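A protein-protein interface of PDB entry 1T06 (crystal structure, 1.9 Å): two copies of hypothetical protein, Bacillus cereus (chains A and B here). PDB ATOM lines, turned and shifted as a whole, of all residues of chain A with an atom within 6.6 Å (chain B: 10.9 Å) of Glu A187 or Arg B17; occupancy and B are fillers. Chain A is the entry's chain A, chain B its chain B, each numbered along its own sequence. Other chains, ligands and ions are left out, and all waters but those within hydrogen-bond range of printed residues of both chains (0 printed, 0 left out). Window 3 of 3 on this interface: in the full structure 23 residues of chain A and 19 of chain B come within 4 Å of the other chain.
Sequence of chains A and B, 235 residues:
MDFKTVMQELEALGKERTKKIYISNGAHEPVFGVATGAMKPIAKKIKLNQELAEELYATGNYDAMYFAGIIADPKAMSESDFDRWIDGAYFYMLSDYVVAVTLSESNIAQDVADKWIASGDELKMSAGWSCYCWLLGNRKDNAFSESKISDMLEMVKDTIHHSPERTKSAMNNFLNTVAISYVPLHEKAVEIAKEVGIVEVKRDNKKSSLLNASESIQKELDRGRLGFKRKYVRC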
ATOM      1  N   ALA A 179     -18.569 -21.244  -8.087  1.00  0.00           N
ATOM      2  CA  ALA A 179     -19.453 -21.832  -7.088  1.00  0.00           C
ATOM      3  C   ALA A 179     -20.457 -20.830  -6.527  1.00  0.00           C
ATOM      4  O   ALA A 179     -21.618 -21.167  -6.290  1.00  0.00           O
ATOM      5  CB  ALA A 179     -18.637 -22.421  -5.955  1.00  0.00           C
ATOM      6  N   VAL A 183     -24.186 -19.719 -10.631  1.00  0.00           N
ATOM      7  CA  VAL A 183     -25.020 -20.803 -10.144  1.00  0.00           C
ATOM      8  C   VAL A 183     -25.308 -21.980 -11.083  1.00  0.00           C
ATOM      9  O   VAL A 183     -25.500 -23.104 -10.607  1.00  0.00           O
ATOM     10  CB  VAL A 183     -26.364 -20.253  -9.594  1.00  0.00           C
ATOM     11  CG1 VAL A 183     -26.087 -19.274  -8.459  1.00  0.00           C
ATOM     12  CG2 VAL A 183     -27.167 -19.581 -10.709  1.00  0.00           C
ATOM     13  N   PRO A 184     -25.356 -21.757 -12.412  1.00  0.00           N
ATOM     14  CA  PRO A 184     -25.632 -22.913 -13.273  1.00  0.00           C
ATOM     15  C   PRO A 184     -24.689 -24.090 -12.999  1.00  0.00           C
ATOM     16  O   PRO A 184     -25.054 -25.247 -13.198  1.00  0.00           O
ATOM     17  CB  PRO A 184     -25.464 -22.339 -14.675  1.00  0.00           C
ATOM     18  CG  PRO A 184     -25.964 -20.939 -14.494  1.00  0.00           C
ATOM     19  CD  PRO A 184     -25.295 -20.521 -13.211  1.00  0.00           C
ATOM     20  N   LEU A 185     -23.485 -23.784 -12.527  1.00  0.00           N
ATOM     21  CA  LEU A 185     -22.492 -24.810 -12.209  1.00  0.00           C
ATOM     22  C   LEU A 185     -22.138 -24.864 -10.725  1.00  0.00           C
ATOM     23  O   LEU A 185     -21.051 -25.325 -10.362  1.00  0.00           O
ATOM     24  CB  LEU A 185     -21.214 -24.585 -13.024  1.00  0.00           C
ATOM     25  CG  LEU A 185     -21.382 -24.808 -14.527  1.00  0.00           C
ATOM     26  CD1 LEU A 185     -20.100 -24.462 -15.263  1.00  0.00           C
ATOM     27  CD2 LEU A 185     -21.788 -26.253 -14.767  1.00  0.00           C
ATOM     28  N   HIS A 186     -23.051 -24.407  -9.867  1.00  0.00           N
ATOM     29  CA  HIS A 186     -22.793 -24.425  -8.433  1.00  0.00           C
ATOM     30  C   HIS A 186     -22.433 -25.806  -7.904  1.00  0.00           C
ATOM     31  O   HIS A 186     -21.410 -25.981  -7.241  1.00  0.00           O
ATOM     32  CB  HIS A 186     -23.993 -23.917  -7.643  1.00  0.00           C
ATOM     33  CG  HIS A 186     -23.803 -24.027  -6.163  1.00  0.00           C
ATOM     34  ND1 HIS A 186     -24.452 -24.969  -5.395  1.00  0.00           N
ATOM     35  CD2 HIS A 186     -22.977 -23.363  -5.322  1.00  0.00           C
ATOM     36  CE1 HIS A 186     -24.033 -24.883  -4.146  1.00  0.00           C
ATOM     37  NE2 HIS A 186     -23.137 -23.916  -4.075  1.00  0.00           N
ATOM     38  N   GLU A 187     -23.283 -26.783  -8.190  1.00  0.00           N
ATOM     39  CA  GLU A 187     -23.045 -28.143  -7.735  1.00  0.00           C
ATOM     40  C   GLU A 187     -21.709 -28.706  -8.217  1.00  0.00           C
ATOM     41  O   GLU A 187     -20.958 -29.280  -7.424  1.00  0.00           O
ATOM     42  CB  GLU A 187     -24.187 -29.059  -8.176  1.00  0.00           C
ATOM     43  CG  GLU A 187     -25.537 -28.801  -7.491  1.00  0.00           C
ATOM     44  CD  GLU A 187     -26.241 -27.550  -7.994  1.00  0.00           C
ATOM     45  OE1 GLU A 187     -26.090 -27.219  -9.191  1.00  0.00           O
ATOM     46  OE2 GLU A 187     -26.965 -26.907  -7.200  1.00  0.00           O
ATOM     47  N   LYS A 188     -21.396 -28.543  -9.499  1.00  0.00           N
ATOM     48  CA  LYS A 188     -20.128 -29.066 -10.021  1.00  0.00           C
ATOM     49  C   LYS A 188     -18.925 -28.400  -9.382  1.00  0.00           C
ATOM     50  O   LYS A 188     -17.952 -29.069  -9.034  1.00  0.00           O
ATOM     51  CB  LYS A 188     -20.022 -28.887 -11.535  1.00  0.00           C
ATOM     52  CG  LYS A 188     -18.784 -29.564 -12.141  1.00  0.00           C
ATOM     53  CD  LYS A 188     -18.678 -29.274 -13.630  1.00  0.00           C
ATOM     54  CE  LYS A 188     -17.646 -30.163 -14.302  1.00  0.00           C
ATOM     55  NZ  LYS A 188     -18.006 -31.599 -14.161  1.00  0.00           N
ATOM     56  N   ALA A 189     -18.983 -27.077  -9.245  1.00  0.00           N
ATOM     57  CA  ALA A 189     -17.883 -26.336  -8.636  1.00  0.00           C
ATOM     58  C   ALA A 189     -17.652 -26.841  -7.211  1.00  0.00           C
ATOM     59  O   ALA A 189     -16.509 -27.028  -6.792  1.00  0.00           O
ATOM     60  CB  ALA A 189     -18.189 -24.837  -8.630  1.00  0.00           C
ATOM     61  N   VAL A 190     -18.738 -27.063  -6.472  1.00  0.00           N
ATOM     62  CA  VAL A 190     -18.638 -27.568  -5.101  1.00  0.00           C
ATOM     63  C   VAL A 190     -18.010 -28.962  -5.098  1.00  0.00           C
ATOM     64  O   VAL A 190     -17.168 -29.291  -4.257  1.00  0.00           O
ATOM     65  CB  VAL A 190     -20.033 -27.651  -4.437  1.00  0.00           C
ATOM     66  CG1 VAL A 190     -19.965 -28.493  -3.169  1.00  0.00           C
ATOM     67  CG2 VAL A 190     -20.535 -26.243  -4.115  1.00  0.00           C
ATOM     68  N   GLU A 191     -18.448 -29.774  -6.050  1.00  0.00           N
ATOM     69  CA  GLU A 191     -17.965 -31.139  -6.211  1.00  0.00           C
ATOM     70  C   GLU A 191     -16.459 -31.126  -6.499  1.00  0.00           C
ATOM     71  O   GLU A 191     -15.687 -31.840  -5.854  1.00  0.00           O
ATOM     72  CB  GLU A 191     -18.760 -31.797  -7.353  1.00  0.00           C
ATOM     73  CG  GLU A 191     -18.119 -32.991  -8.053  1.00  0.00           C
ATOM     74  CD  GLU A 191     -18.581 -33.109  -9.514  1.00  0.00           C
ATOM     75  OE1 GLU A 191     -19.815 -33.168  -9.751  1.00  0.00           O
ATOM     76  OE2 GLU A 191     -17.709 -33.132 -10.423  1.00  0.00           O
ATOM     77  N   ILE A 192     -16.037 -30.299  -7.452  1.00  0.00           N
ATOM     78  CA  ILE A 192     -14.622 -30.216  -7.797  1.00  0.00           C
ATOM     79  C   ILE A 192     -13.741 -29.627  -6.683  1.00  0.00           C
ATOM     80  O   ILE A 192     -12.601 -30.052  -6.511  1.00  0.00           O
ATOM     81  CB  ILE A 192     -14.426 -29.417  -9.100  1.00  0.00           C
ATOM     82  CG1 ILE A 192     -14.914 -30.260 -10.283  1.00  0.00           C
ATOM     83  CG2 ILE A 192     -12.959 -29.027  -9.274  1.00  0.00           C
ATOM     84  CD1 ILE A 192     -14.778 -29.574 -11.625  1.00  0.00           C
ATOM     85  N   LEU A 226     -25.040 -17.112  -2.122  1.00  0.00           N
ATOM     86  CA  LEU A 226     -25.092 -17.904  -3.350  1.00  0.00           C
ATOM     87  C   LEU A 226     -25.763 -17.045  -4.427  1.00  0.00           C
ATOM     88  O   LEU A 226     -26.835 -16.471  -4.192  1.00  0.00           O
ATOM     89  CB  LEU A 226     -25.917 -19.172  -3.149  1.00  0.00           C
ATOM     90  CG  LEU A 226     -26.136 -19.941  -4.453  1.00  0.00           C
ATOM     91  CD1 LEU A 226     -24.836 -20.632  -4.842  1.00  0.00           C
ATOM     92  CD2 LEU A 226     -27.274 -20.950  -4.289  1.00  0.00           C
ATOM     93  N   LEU B  13     -39.783 -15.137  -7.754  1.00  0.00           N
ATOM     94  CA  LEU B  13     -38.323 -15.162  -7.791  1.00  0.00           C
ATOM     95  C   LEU B  13     -37.694 -16.328  -7.035  1.00  0.00           C
ATOM     96  O   LEU B  13     -36.508 -16.612  -7.204  1.00  0.00           O
ATOM     97  CB  LEU B  13     -37.763 -13.854  -7.237  1.00  0.00           C
ATOM     98  CG  LEU B  13     -37.978 -12.618  -8.099  1.00  0.00           C
ATOM     99  CD1 LEU B  13     -37.531 -11.388  -7.335  1.00  0.00           C
ATOM    100  CD2 LEU B  13     -37.186 -12.758  -9.380  1.00  0.00           C
ATOM    101  N   GLY B  14     -38.482 -16.994  -6.198  1.00  0.00           N
ATOM    102  CA  GLY B  14     -37.963 -18.114  -5.432  1.00  0.00           C
ATOM    103  C   GLY B  14     -37.410 -19.243  -6.288  1.00  0.00           C
ATOM    104  O   GLY B  14     -37.954 -19.571  -7.342  1.00  0.00           O
ATOM    105  N   LYS B  15     -36.315 -19.835  -5.836  1.00  0.00           N
ATOM    106  CA  LYS B  15     -35.705 -20.942  -6.551  1.00  0.00           C
ATOM    107  C   LYS B  15     -35.270 -21.963  -5.519  1.00  0.00           C
ATOM    108  O   LYS B  15     -34.801 -21.613  -4.435  1.00  0.00           O
ATOM    109  CB  LYS B  15     -34.526 -20.450  -7.387  1.00  0.00           C
ATOM    110  CG  LYS B  15     -34.956 -19.419  -8.416  1.00  0.00           C
ATOM    111  CD  LYS B  15     -33.797 -18.872  -9.218  1.00  0.00           C
ATOM    112  CE  LYS B  15     -34.100 -17.453  -9.711  1.00  0.00           C
ATOM    113  NZ  LYS B  15     -35.449 -17.315 -10.353  1.00  0.00           N
ATOM    114  N   GLU B  16     -35.442 -23.232  -5.863  1.00  0.00           N
ATOM    115  CA  GLU B  16     -35.130 -24.328  -4.965  1.00  0.00           C
ATOM    116  C   GLU B  16     -33.699 -24.371  -4.437  1.00  0.00           C
ATOM    117  O   GLU B  16     -33.476 -24.619  -3.250  1.00  0.00           O
ATOM    118  CB  GLU B  16     -35.481 -25.649  -5.650  1.00  0.00           C
ATOM    119  CG  GLU B  16     -35.635 -26.802  -4.678  1.00  0.00           C
ATOM    120  CD  GLU B  16     -36.480 -26.433  -3.458  1.00  0.00           C
ATOM    121  OE1 GLU B  16     -37.635 -25.966  -3.636  1.00  0.00           O
ATOM    122  OE2 GLU B  16     -35.980 -26.614  -2.322  1.00  0.00           O
ATOM    123  N   ARG B  17     -32.729 -24.127  -5.311  1.00  0.00           N
ATOM    124  CA  ARG B  17     -31.335 -24.167  -4.894  1.00  0.00           C
ATOM    125  C   ARG B  17     -31.071 -23.184  -3.753  1.00  0.00           C
ATOM    126  O   ARG B  17     -30.430 -23.527  -2.761  1.00  0.00           O
ATOM    127  CB  ARG B  17     -30.423 -23.857  -6.081  1.00  0.00           C
ATOM    128  CG  ARG B  17     -28.949 -23.996  -5.773  1.00  0.00           C
ATOM    129  CD  ARG B  17     -28.118 -23.434  -6.905  1.00  0.00           C
ATOM    130  NE  ARG B  17     -27.897 -24.402  -7.972  1.00  0.00           N
ATOM    131  CZ  ARG B  17     -28.170 -24.178  -9.251  1.00  0.00           C
ATOM    132  NH1 ARG B  17     -28.687 -23.014  -9.628  1.00  0.00           N
ATOM    133  NH2 ARG B  17     -27.913 -25.112 -10.157  1.00  0.00           N
ATOM    134  N   THR B  18     -31.578 -21.965  -3.904  1.00  0.00           N
ATOM    135  CA  THR B  18     -31.419 -20.913  -2.905  1.00  0.00           C
ATOM    136  C   THR B  18     -32.162 -21.276  -1.617  1.00  0.00           C
ATOM    137  O   THR B  18     -31.628 -21.144  -0.513  1.00  0.00           O
ATOM    138  CB  THR B  18     -31.973 -19.581  -3.448  1.00  0.00           C
ATOM    139  OG1 THR B  18     -31.295 -19.253  -4.663  1.00  0.00           O
ATOM    140  CG2 THR B  18     -31.779 -18.457  -2.443  1.00  0.00           C
ATOM    141  N   LYS B  19     -33.401 -21.736  -1.775  1.00  0.00           N
ATOM    142  CA  LYS B  19     -34.248 -22.123  -0.651  1.00  0.00           C
ATOM    143  C   LYS B  19     -33.593 -23.225   0.193  1.00  0.00           C
ATOM    144  O   LYS B  19     -33.531 -23.139   1.421  1.00  0.00           O
ATOM    145  CB  LYS B  19     -35.602 -22.600  -1.187  1.00  0.00           C
ATOM    146  CG  LYS B  19     -36.626 -22.946  -0.123  1.00  0.00           C
ATOM    147  CD  LYS B  19     -37.916 -23.473  -0.750  1.00  0.00           C
ATOM    148  CE  LYS B  19     -38.963 -23.780   0.308  1.00  0.00           C
ATOM    149  NZ  LYS B  19     -40.246 -24.222  -0.303  1.00  0.00           N
ATOM    150  N   LYS B  20     -33.104 -24.258  -0.478  1.00  0.00           N
ATOM    151  CA  LYS B  20     -32.462 -25.370   0.198  1.00  0.00           C
ATOM    152  C   LYS B  20     -31.374 -24.880   1.142  1.00  0.00           C
ATOM    153  O   LYS B  20     -31.285 -25.314   2.296  1.00  0.00           O
ATOM    154  CB  LYS B  20     -31.863 -26.314  -0.841  1.00  0.00           C
ATOM    155  CG  LYS B  20     -31.284 -27.588  -0.275  1.00  0.00           C
ATOM    156  CD  LYS B  20     -30.865 -28.526  -1.403  1.00  0.00           C
ATOM    157  CE  LYS B  20     -30.431 -29.884  -0.863  1.00  0.00           C
ATOM    158  NZ  LYS B  20     -30.293 -30.898  -1.953  1.00  0.00           N
ATOM    159  N   ILE B  21     -30.545 -23.968   0.651  1.00  0.00           N
ATOM    160  CA  ILE B  21     -29.454 -23.432   1.453  1.00  0.00           C
ATOM    161  C   ILE B  21     -29.940 -22.590   2.626  1.00  0.00           C
ATOM    162  O   ILE B  21     -29.404 -22.684   3.726  1.00  0.00           O
ATOM    163  CB  ILE B  21     -28.505 -22.628   0.568  1.00  0.00           C
ATOM    164  CG1 ILE B  21     -27.797 -23.596  -0.383  1.00  0.00           C
ATOM    165  CG2 ILE B  21     -27.495 -21.868   1.416  1.00  0.00           C
ATOM    166  CD1 ILE B  21     -26.967 -22.921  -1.435  1.00  0.00           C
ATOM    167  N   TYR B  22     -30.963 -21.775   2.400  1.00  0.00           N
ATOM    168  CA  TYR B  22     -31.505 -20.965   3.480  1.00  0.00           C
ATOM    169  C   TYR B  22     -32.002 -21.862   4.614  1.00  0.00           C
ATOM    170  O   TYR B  22     -31.740 -21.599   5.786  1.00  0.00           O
ATOM    171  CB  TYR B  22     -32.658 -20.096   2.970  1.00  0.00           C
ATOM    172  CG  TYR B  22     -32.225 -18.874   2.188  1.00  0.00           C
ATOM    173  CD1 TYR B  22     -30.874 -18.527   2.075  1.00  0.00           C
ATOM    174  CD2 TYR B  22     -33.171 -18.048   1.576  1.00  0.00           C
ATOM    175  CE1 TYR B  22     -30.478 -17.387   1.371  1.00  0.00           C
ATOM    176  CE2 TYR B  22     -32.786 -16.911   0.871  1.00  0.00           C
ATOM    177  CZ  TYR B  22     -31.440 -16.585   0.770  1.00  0.00           C
ATOM    178  OH  TYR B  22     -31.062 -15.467   0.056  1.00  0.00           O
ATOM    179  N   ILE B  23     -32.728 -22.919   4.259  1.00  0.00           N
ATOM    180  CA  ILE B  23     -33.265 -23.852   5.257  1.00  0.00           C
ATOM    181  C   ILE B  23     -32.115 -24.576   5.955  1.00  0.00           C
ATOM    182  O   ILE B  23     -32.180 -24.873   7.148  1.00  0.00           O
ATOM    183  CB  ILE B  23     -34.251 -24.866   4.594  1.00  0.00           C
ATOM    184  CG1 ILE B  23     -35.508 -24.111   4.138  1.00  0.00           C
ATOM    185  CG2 ILE B  23     -34.609 -25.979   5.565  1.00  0.00           C
ATOM    186  CD1 ILE B  23     -36.515 -24.951   3.377  1.00  0.00           C
ATOM    187  N   SER B  24     -31.055 -24.842   5.205  1.00  0.00           N
ATOM    188  CA  SER B  24     -29.877 -25.481   5.765  1.00  0.00           C
ATOM    189  C   SER B  24     -29.253 -24.537   6.810  1.00  0.00           C
ATOM    190  O   SER B  24     -28.717 -24.982   7.823  1.00  0.00           O
ATOM    191  CB  SER B  24     -28.873 -25.772   4.647  1.00  0.00           C
ATOM    192  OG  SER B  24     -27.694 -26.350   5.168  1.00  0.00           O
ATOM    193  N   ASN B  25     -29.329 -23.230   6.562  1.00  0.00           N
ATOM    194  CA  ASN B  25     -28.776 -22.247   7.492  1.00  0.00           C
ATOM    195  C   ASN B  25     -29.666 -22.042   8.718  1.00  0.00           C
ATOM    196  O   ASN B  25     -29.246 -21.419   9.696  1.00  0.00           O
ATOM    197  CB  ASN B  25     -28.566 -20.888   6.803  1.00  0.00           C
ATOM    198  CG  ASN B  25     -27.475 -20.923   5.748  1.00  0.00           C
ATOM    199  OD1 ASN B  25     -26.726 -21.894   5.649  1.00  0.00           O
ATOM    200  ND2 ASN B  25     -27.373 -19.849   4.961  1.00  0.00           N
ATOM    201  N   ALA B  27     -33.431 -21.395   8.286  1.00  0.00           N
ATOM    202  CA  ALA B  27     -34.764 -20.893   7.969  1.00  0.00           C
ATOM    203  C   ALA B  27     -35.738 -22.060   7.920  1.00  0.00           C
ATOM    204  O   ALA B  27     -35.337 -23.209   7.698  1.00  0.00           O
ATOM    205  CB  ALA B  27     -34.759 -20.178   6.628  1.00  0.00           C
ATOM    206  N   VAL B  31     -40.910 -20.015   3.206  1.00  0.00           N
ATOM    207  CA  VAL B  31     -39.730 -19.388   2.618  1.00  0.00           C
ATOM    208  C   VAL B  31     -39.668 -19.712   1.117  1.00  0.00           C
ATOM    209  O   VAL B  31     -39.900 -20.854   0.706  1.00  0.00           O
ATOM    210  CB  VAL B  31     -38.429 -19.883   3.330  1.00  0.00           C
ATOM    211  CG1 VAL B  31     -38.291 -21.397   3.187  1.00  0.00           C
ATOM    212  CG2 VAL B  31     -37.214 -19.183   2.758  1.00  0.00           C
ATOM    213  N   PHE B  32     -39.364 -18.705   0.302  1.00  0.00           N
ATOM    214  CA  PHE B  32     -39.280 -18.891  -1.148  1.00  0.00           C
ATOM    215  C   PHE B  32     -37.862 -19.192  -1.644  1.00  0.00           C
ATOM    216  O   PHE B  32     -37.682 -19.965  -2.584  1.00  0.00           O
ATOM    217  CB  PHE B  32     -39.782 -17.646  -1.892  1.00  0.00           C
ATOM    218  CG  PHE B  32     -41.155 -17.187  -1.485  1.00  0.00           C
ATOM    219  CD1 PHE B  32     -42.202 -18.096  -1.336  1.00  0.00           C
ATOM    220  CD2 PHE B  32     -41.413 -15.831  -1.299  1.00  0.00           C
ATOM    221  CE1 PHE B  32     -43.499 -17.657  -1.008  1.00  0.00           C
ATOM    222  CE2 PHE B  32     -42.696 -15.378  -0.973  1.00  0.00           C
ATOM    223  CZ  PHE B  32     -43.744 -16.292  -0.828  1.00  0.00           C
ATOM    224  N   GLY B  33     -36.864 -18.566  -1.022  1.00  0.00           N
ATOM    225  CA  GLY B  33     -35.487 -18.764  -1.441  1.00  0.00           C
ATOM    226  C   GLY B  33     -35.149 -17.771  -2.538  1.00  0.00           C
ATOM    227  O   GLY B  33     -34.788 -18.153  -3.652  1.00  0.00           O
ATOM    228  N   VAL B  34     -35.267 -16.487  -2.214  1.00  0.00           N
ATOM    229  CA  VAL B  34     -35.003 -15.404  -3.159  1.00  0.00           C
ATOM    230  C   VAL B  34     -33.569 -14.865  -3.090  1.00  0.00           C
ATOM    231  O   VAL B  34     -33.050 -14.609  -2.001  1.00  0.00           O
ATOM    232  CB  VAL B  34     -35.986 -14.215  -2.911  1.00  0.00           C
ATOM    233  CG1 VAL B  34     -35.612 -13.024  -3.799  1.00  0.00           C
ATOM    234  CG2 VAL B  34     -37.422 -14.653  -3.180  1.00  0.00           C
ATOM    235  N   ALA B  35     -32.935 -14.696  -4.252  1.00  0.00           N
ATOM    236  CA  ALA B  35     -31.573 -14.161  -4.316  1.00  0.00           C
ATOM    237  C   ALA B  35     -31.695 -12.663  -4.054  1.00  0.00           C
ATOM    238  O   ALA B  35     -32.480 -11.985  -4.709  1.00  0.00           O
ATOM    239  CB  ALA B  35     -30.970 -14.413  -5.692  1.00  0.00           C
ATOM    240  N   ASP B  63     -37.776 -14.447   3.201  1.00  0.00           N
ATOM    241  CA  ASP B  63     -37.559 -13.538   2.077  1.00  0.00           C
ATOM    242  C   ASP B  63     -38.346 -12.241   2.226  1.00  0.00           C
ATOM    243  O   ASP B  63     -37.826 -11.160   1.952  1.00  0.00           O
ATOM    244  CB  ASP B  63     -37.941 -14.228   0.775  1.00  0.00           C
ATOM    245  CG  ASP B  63     -37.175 -15.516   0.561  1.00  0.00           C
ATOM    246  OD1 ASP B  63     -35.939 -15.456   0.362  1.00  0.00           O
ATOM    247  OD2 ASP B  63     -37.805 -16.592   0.604  1.00  0.00           O
ATOM    248  N   MET B  93     -29.659 -15.474  10.268  1.00  0.00           N
ATOM    249  CA  MET B  93     -29.757 -14.680   9.040  1.00  0.00           C
ATOM    250  C   MET B  93     -30.697 -13.497   9.264  1.00  0.00           C
ATOM    251  O   MET B  93     -30.505 -12.423   8.694  1.00  0.00           O
ATOM    252  CB  MET B  93     -30.247 -15.524   7.852  1.00  0.00           C
ATOM    253  CG  MET B  93     -29.232 -16.575   7.330  1.00  0.00           C
ATOM    254  SD  MET B  93     -29.747 -17.377   5.766  1.00  0.00           S
ATOM    255  CE  MET B  93     -29.265 -16.179   4.606  1.00  0.00           C
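The guanidinium group of Arg B17 lies within hydrogen-bond range of the backbone carbonyl oxygen of Val A183 (3.2 Å).
The side-chain carboxylate (OE2) of Glu A187 lies within salt-bridge range of the guanidinium group (NE) of Arg B17, at 2.8 Å.
The backbone carbonyl oxygen of Ile B21 lies close to the side-chain amide oxygen of Asn B25, at 3.4 Å.
CB of His A186 touches NE of Arg B17 (3.9 Å).
Leu A226 touches Arg B17 (CD2 to CD, 3.7 Å).
Leu A226 touches Ile B21.
Val A183 touches just one residue of chain B: Arg B17.
Of chain B, only Arg B17 (3.9 Å) comes within 4 Å of His A186.
No residue of chain B comes within 4 Å of Ala A189.
No residue of chain B comes within 4 Å of Glu A191.
Of the printed residues of chain B, Leu A226 touches Arg B17 (3.7 Å) and Ile B21 (3.5 Å).
Of the printed residues of chain A, Arg B17 touches Val A183 (3.2 Å), His A186 (3.9 Å), Glu A187 (2.8 Å) and Leu A226 (3.7 Å).
Printed residues of chain A within 4 Å of Ile B21: Leu A226.
The nearest residue of chain B that does not touch Glu A187 is Ile B21 (7.0 Å).
Hydrophobic or aromatic side chains of chain B within 4 Å of the printed part of chain A: Ile B21.
Of the 12 printed residues of chain A, 4 touch a printed residue of chain B.
Hydrophobic or aromatic side chains of chain A within 4 Å of the printed part of chain B: Val A183, His A186 and Leu A226.
No position is printed for both chains.
Of the 5 pairs that touch across the chains among the printed residues, none has its exchanged pair printed and touching as well.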
